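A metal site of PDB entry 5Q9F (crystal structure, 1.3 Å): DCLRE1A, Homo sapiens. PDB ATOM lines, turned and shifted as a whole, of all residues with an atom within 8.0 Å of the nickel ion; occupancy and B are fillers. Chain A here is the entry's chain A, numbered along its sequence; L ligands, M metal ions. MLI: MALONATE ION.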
ATOM      1  N   ASP A  18      -9.660  27.038  20.210  1.00  0.00           N
ATOM      2  CA  ASP A  18     -10.862  26.405  20.811  1.00  0.00           C
ATOM      3  C   ASP A  18     -10.793  26.331  22.382  1.00  0.00           C
ATOM      4  O   ASP A  18     -11.151  25.309  22.989  1.00  0.00           O
ATOM      5  CB  ASP A  18     -11.213  25.086  20.149  1.00  0.00           C
ATOM      6  CG  ASP A  18     -11.435  25.219  18.607  1.00  0.00           C
ATOM      7  OD1 ASP A  18     -11.599  26.365  18.128  1.00  0.00           O
ATOM      8  OD2 ASP A  18     -11.445  24.104  17.994  1.00  0.00           O
ATOM      9  N   THR A  34     -12.081  27.398  15.542  1.00  0.00           N
ATOM     10  CA  THR A  34     -12.110  26.613  14.299  1.00  0.00           C
ATOM     11  C   THR A  34     -13.486  26.497  13.647  1.00  0.00           C
ATOM     12  O   THR A  34     -13.589  26.506  12.400  1.00  0.00           O
ATOM     13  CB  THR A  34     -11.456  25.243  14.438  1.00  0.00           C
ATOM     14  OG1 THR A  34     -12.225  24.412  15.356  1.00  0.00           O
ATOM     15  CG2 THR A  34      -9.973  25.287  14.871  1.00  0.00           C
ATOM     16  N   HIS A  35     -14.519  26.375  14.503  1.00  0.00           N
ATOM     17  CA  HIS A  35     -15.890  26.168  14.002  1.00  0.00           C
ATOM     18  C   HIS A  35     -16.893  26.365  15.099  1.00  0.00           C
ATOM     19  O   HIS A  35     -16.570  26.237  16.310  1.00  0.00           O
ATOM     20  CB  HIS A  35     -16.038  24.770  13.275  1.00  0.00           C
ATOM     21  CG  HIS A  35     -15.946  23.568  14.186  1.00  0.00           C
ATOM     22  ND1 HIS A  35     -14.776  23.144  14.788  1.00  0.00           N
ATOM     23  CD2 HIS A  35     -16.881  22.652  14.512  1.00  0.00           C
ATOM     24  CE1 HIS A  35     -15.059  22.030  15.488  1.00  0.00           C
ATOM     25  NE2 HIS A  35     -16.278  21.692  15.255  1.00  0.00           N
ATOM     26  N   PHE A  36     -18.144  26.581  14.681  1.00  0.00           N
ATOM     27  CA  PHE A  36     -19.262  26.839  15.641  1.00  0.00           C
ATOM     28  C   PHE A  36     -19.957  25.541  16.083  1.00  0.00           C
ATOM     29  O   PHE A  36     -21.187  25.304  15.762  1.00  0.00           O
ATOM     30  CB  PHE A  36     -20.264  27.803  14.967  1.00  0.00           C
ATOM     31  CG  PHE A  36     -21.263  28.478  15.915  1.00  0.00           C
ATOM     32  CD1 PHE A  36     -20.840  29.488  16.764  1.00  0.00           C
ATOM     33  CD2 PHE A  36     -22.576  28.041  16.018  1.00  0.00           C
ATOM     34  CE1 PHE A  36     -21.741  30.120  17.663  1.00  0.00           C
ATOM     35  CE2 PHE A  36     -23.499  28.676  16.891  1.00  0.00           C
ATOM     36  CZ  PHE A  36     -23.076  29.670  17.706  1.00  0.00           C
ATOM     37  N   HIS A  37     -19.249  24.679  16.836  1.00  0.00           N
ATOM     38  CA  HIS A  37     -19.820  23.541  17.594  1.00  0.00           C
ATOM     39  C   HIS A  37     -19.581  23.817  19.100  1.00  0.00           C
ATOM     40  O   HIS A  37     -18.499  24.296  19.517  1.00  0.00           O
ATOM     41  CB  HIS A  37     -19.244  22.179  17.167  1.00  0.00           C
ATOM     42  CG  HIS A  37     -19.813  21.607  15.899  1.00  0.00           C
ATOM     43  ND1 HIS A  37     -19.244  20.560  15.184  1.00  0.00           N
ATOM     44  CD2 HIS A  37     -21.021  21.847  15.317  1.00  0.00           C
ATOM     45  CE1 HIS A  37     -20.024  20.256  14.138  1.00  0.00           C
ATOM     46  NE2 HIS A  37     -21.080  21.063  14.183  1.00  0.00           N
ATOM     47  N   SER A  38     -20.570  23.420  19.936  1.00  0.00           N
ATOM     48  CA  SER A  38     -20.594  23.895  21.339  1.00  0.00           C
ATOM     49  C   SER A  38     -19.398  23.420  22.155  1.00  0.00           C
ATOM     50  O   SER A  38     -18.927  24.248  22.992  1.00  0.00           O
ATOM     51  CB  SER A  38     -21.951  23.594  21.967  1.00  0.00           C
ATOM     52  OG  SER A  38     -22.146  22.195  22.020  1.00  0.00           O
ATOM     53  N   ASP A  39     -18.857  22.233  21.908  1.00  0.00           N
ATOM     54  CA  ASP A  39     -17.686  21.746  22.706  1.00  0.00           C
ATOM     55  C   ASP A  39     -16.470  22.641  22.417  1.00  0.00           C
ATOM     56  O   ASP A  39     -15.499  22.684  23.207  1.00  0.00           O
ATOM     57  CB  ASP A  39     -17.312  20.308  22.407  1.00  0.00           C
ATOM     58  CG  ASP A  39     -18.184  19.214  23.150  1.00  0.00           C
ATOM     59  OD1 ASP A  39     -19.040  19.598  23.961  1.00  0.00           O
ATOM     60  OD2 ASP A  39     -17.966  18.034  22.855  1.00  0.00           O
ATOM     61  N   HIS A  40     -16.449  23.311  21.255  1.00  0.00           N
ATOM     62  CA  HIS A  40     -15.359  24.227  20.849  1.00  0.00           C
ATOM     63  C   HIS A  40     -15.551  25.670  21.177  1.00  0.00           C
ATOM     64  O   HIS A  40     -14.577  26.355  21.577  1.00  0.00           O
ATOM     65  CB  HIS A  40     -15.136  23.999  19.286  1.00  0.00           C
ATOM     66  CG  HIS A  40     -14.751  22.615  18.969  1.00  0.00           C
ATOM     67  ND1 HIS A  40     -13.457  22.210  18.706  1.00  0.00           N
ATOM     68  CD2 HIS A  40     -15.495  21.474  18.868  1.00  0.00           C
ATOM     69  CE1 HIS A  40     -13.415  20.933  18.459  1.00  0.00           C
ATOM     70  NE2 HIS A  40     -14.649  20.447  18.571  1.00  0.00           N
ATOM     71  N   HIS A  96     -15.752  19.964   7.212  1.00  0.00           N
ATOM     72  CA  HIS A  96     -16.503  19.589   8.447  1.00  0.00           C
ATOM     73  C   HIS A  96     -17.881  20.192   8.290  1.00  0.00           C
ATOM     74  O   HIS A  96     -18.611  19.756   7.355  1.00  0.00           O
ATOM     75  CB  HIS A  96     -15.742  19.956   9.708  1.00  0.00           C
ATOM     76  CG  HIS A  96     -16.306  19.522  11.055  1.00  0.00           C
ATOM     77  ND1 HIS A  96     -16.714  18.242  11.313  1.00  0.00           N
ATOM     78  CD2 HIS A  96     -16.597  20.268  12.138  1.00  0.00           C
ATOM     79  CE1 HIS A  96     -17.184  18.209  12.567  1.00  0.00           C
ATOM     80  NE2 HIS A  96     -17.089  19.397  13.118  1.00  0.00           N
ATOM     81  N   CYS A  97     -18.337  21.088   9.126  1.00  0.00           N
ATOM     82  CA  CYS A  97     -19.610  21.833   9.008  1.00  0.00           C
ATOM     83  C   CYS A  97     -19.375  23.172   8.318  1.00  0.00           C
ATOM     84  O   CYS A  97     -18.237  23.598   8.186  1.00  0.00           O
ATOM     85  CB  CYS A  97     -20.194  21.964  10.445  1.00  0.00           C
ATOM     86  SG  CYS A  97     -19.199  23.037  11.554  1.00  0.00           S
ATOM     87  N   ALA A 100     -16.224  25.796   9.037  1.00  0.00           N
ATOM     88  CA  ALA A 100     -15.143  25.092   9.734  1.00  0.00           C
ATOM     89  C   ALA A 100     -13.804  25.223   8.998  1.00  0.00           C
ATOM     90  O   ALA A 100     -13.772  24.998   7.778  1.00  0.00           O
ATOM     91  CB  ALA A 100     -15.515  23.675   9.964  1.00  0.00           C
ATOM     92  N   GLY A 117      -8.442  21.513  13.468  1.00  0.00           N
ATOM     93  CA  GLY A 117      -9.764  21.628  14.076  1.00  0.00           C
ATOM     94  C   GLY A 117     -10.438  20.283  13.963  1.00  0.00           C
ATOM     95  O   GLY A 117      -9.810  19.235  14.104  1.00  0.00           O
ATOM     96  N   ASP A 118     -11.768  20.295  13.791  1.00  0.00           N
ATOM     97  CA  ASP A 118     -12.495  19.084  13.349  1.00  0.00           C
ATOM     98  C   ASP A 118     -12.492  19.016  11.788  1.00  0.00           C
ATOM     99  O   ASP A 118     -12.725  20.037  11.135  1.00  0.00           O
ATOM    100  CB  ASP A 118     -13.921  19.024  13.850  1.00  0.00           C
ATOM    101  CG  ASP A 118     -14.106  18.692  15.340  1.00  0.00           C
ATOM    102  OD1 ASP A 118     -13.166  18.200  15.972  1.00  0.00           O
ATOM    103  OD2 ASP A 118     -15.272  18.746  15.804  1.00  0.00           O
ATOM    104  N   PHE A 119     -12.183  17.833  11.242  1.00  0.00           N
ATOM    105  CA  PHE A 119     -12.101  17.708   9.750  1.00  0.00           C
ATOM    106  C   PHE A 119     -12.508  16.365   9.248  1.00  0.00           C
ATOM    107  O   PHE A 119     -12.448  15.370   9.993  1.00  0.00           O
ATOM    108  CB  PHE A 119     -10.691  18.197   9.168  1.00  0.00           C
ATOM    109  CG  PHE A 119      -9.552  17.171   9.122  1.00  0.00           C
ATOM    110  CD1 PHE A 119      -8.669  17.111   8.034  1.00  0.00           C
ATOM    111  CD2 PHE A 119      -9.293  16.269  10.176  1.00  0.00           C
ATOM    112  CE1 PHE A 119      -7.603  16.258   8.045  1.00  0.00           C
ATOM    113  CE2 PHE A 119      -8.238  15.345  10.141  1.00  0.00           C
ATOM    114  CZ  PHE A 119      -7.391  15.362   9.049  1.00  0.00           C
ATOM    115  N   ASP A 141      -7.431  15.973  14.517  1.00  0.00           N
ATOM    116  CA  ASP A 141      -8.763  15.412  14.915  1.00  0.00           C
ATOM    117  C   ASP A 141      -8.689  13.923  14.699  1.00  0.00           C
ATOM    118  O   ASP A 141      -8.803  13.359  13.603  1.00  0.00           O
ATOM    119  CB  ASP A 141      -9.831  16.049  14.032  1.00  0.00           C
ATOM    120  CG  ASP A 141     -11.209  15.382  14.151  1.00  0.00           C
ATOM    121  OD1 ASP A 141     -11.377  14.532  15.071  1.00  0.00           O
ATOM    122  OD2 ASP A 141     -12.041  15.611  13.244  1.00  0.00           O
ATOM    123  N   THR A 143     -10.951  11.724  16.143  1.00  0.00           N
ATOM    124  CA  THR A 143     -12.229  11.177  16.555  1.00  0.00           C
ATOM    125  C   THR A 143     -12.365   9.694  16.242  1.00  0.00           C
ATOM    126  O   THR A 143     -12.733   8.893  17.148  1.00  0.00           O
ATOM    127  CB  THR A 143     -13.395  11.983  15.911  1.00  0.00           C
ATOM    128  OG1 THR A 143     -13.389  13.350  16.361  1.00  0.00           O
ATOM    129  CG2 THR A 143     -14.766  11.380  16.293  1.00  0.00           C
ATOM    130  N   SER A 183     -27.210  20.755  15.845  1.00  0.00           N
ATOM    131  CA  SER A 183     -26.038  21.608  15.663  1.00  0.00           C
ATOM    132  C   SER A 183     -25.999  21.947  14.174  1.00  0.00           C
ATOM    133  O   SER A 183     -26.673  21.269  13.363  1.00  0.00           O
ATOM    134  CB  SER A 183     -24.725  20.902  16.025  1.00  0.00           C
ATOM    135  OG  SER A 183     -24.542  19.720  15.265  1.00  0.00           O
ATOM    136  N   ILE A 184     -25.216  22.901  13.750  1.00  0.00           N
ATOM    137  CA  ILE A 184     -24.924  23.031  12.341  1.00  0.00           C
ATOM    138  C   ILE A 184     -24.084  21.857  11.818  1.00  0.00           C
ATOM    139  O   ILE A 184     -23.509  21.046  12.645  1.00  0.00           O
ATOM    140  CB  ILE A 184     -24.164  24.343  11.998  1.00  0.00           C
ATOM    141  CG1 ILE A 184     -22.749  24.439  12.572  1.00  0.00           C
ATOM    142  CG2 ILE A 184     -25.044  25.541  12.371  1.00  0.00           C
ATOM    143  CD1 ILE A 184     -21.909  25.565  12.005  1.00  0.00           C
ATOM    144  N   GLU A 296     -19.154  13.805   9.240  1.00  0.00           N
ATOM    145  CA  GLU A 296     -18.315  15.002   9.007  1.00  0.00           C
ATOM    146  C   GLU A 296     -16.909  14.947   9.697  1.00  0.00           C
ATOM    147  O   GLU A 296     -16.202  15.965   9.840  1.00  0.00           O
ATOM    148  CB  GLU A 296     -19.033  16.308   9.259  1.00  0.00           C
ATOM    149  CG  GLU A 296     -20.223  16.546   8.234  1.00  0.00           C
ATOM    150  CD  GLU A 296     -20.917  17.900   8.344  1.00  0.00           C
ATOM    151  OE1 GLU A 296     -20.893  18.556   9.416  1.00  0.00           O
ATOM    152  OE2 GLU A 296     -21.609  18.229   7.319  1.00  0.00           O
ATOM    153  N   HIS A 297     -16.521  13.699  10.050  1.00  0.00           N
ATOM    154  CA  HIS A 297     -15.154  13.416  10.471  1.00  0.00           C
ATOM    155  C   HIS A 297     -14.503  12.334   9.612  1.00  0.00           C
ATOM    156  O   HIS A 297     -15.193  11.461   9.052  1.00  0.00           O
ATOM    157  CB  HIS A 297     -15.070  12.918  11.967  1.00  0.00           C
ATOM    158  CG  HIS A 297     -15.537  13.896  12.982  1.00  0.00           C
ATOM    159  ND1 HIS A 297     -14.715  14.821  13.569  1.00  0.00           N
ATOM    160  CD2 HIS A 297     -16.759  14.029  13.594  1.00  0.00           C
ATOM    161  CE1 HIS A 297     -15.410  15.525  14.484  1.00  0.00           C
ATOM    162  NE2 HIS A 297     -16.628  15.053  14.487  1.00  0.00           N
HETATM  163  C1  MLI L   1     -19.126  17.859  17.457  1.00  0.00           C
HETATM  164  C2  MLI L   1     -18.622  16.970  16.269  1.00  0.00           C
HETATM  165  C3  MLI L   1     -18.034  18.725  18.134  1.00  0.00           C
HETATM  166  O6  MLI L   1     -18.781  15.747  16.145  1.00  0.00           O
HETATM  167  O7  MLI L   1     -18.053  17.591  15.384  1.00  0.00           O
HETATM  168  O8  MLI L   1     -17.388  19.493  17.417  1.00  0.00           O
HETATM  169  O9  MLI L   1     -17.955  18.748  19.392  1.00  0.00           O
HETATM  170 NI    NI M   1     -17.221  19.635  15.359  1.00  0.00          NI
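The nickel ion is bound by an oxygen (O8) of the ligand (2.1 Å), the side-chain carboxylate (OD2) of Asp 118 (2.2 Å), an oxygen (O7) of the ligand (2.2 Å), a ring nitrogen (ND1) of His 37 (2.2 Å), a ring nitrogen (NE2) of His 96 (2.3 Å) and a ring nitrogen (NE2) of His 35 (2.3 Å).
A ring nitrogen (NE2) of His 40 lies close to the side-chain carboxylate (OD2) of Asp 118 (3.3 Å).
The side-chain sulfur (SG) of Cys 97 sits at hydrogen-bond distance from a ring nitrogen (NE2) of His 37, 3.8 Å away.
The backbone carbonyl oxygen (O) of Ile 184 is in hydrogen-bond range of a ring nitrogen (NE2) of His 37 (2.9 Å).
ND1 of His 96 is in hydrogen-bond range of O of Glu 296 (2.8 Å).
ND1 of His 35 sits at hydrogen-bond distance from OG1 of Thr 34, 2.9 Å away.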
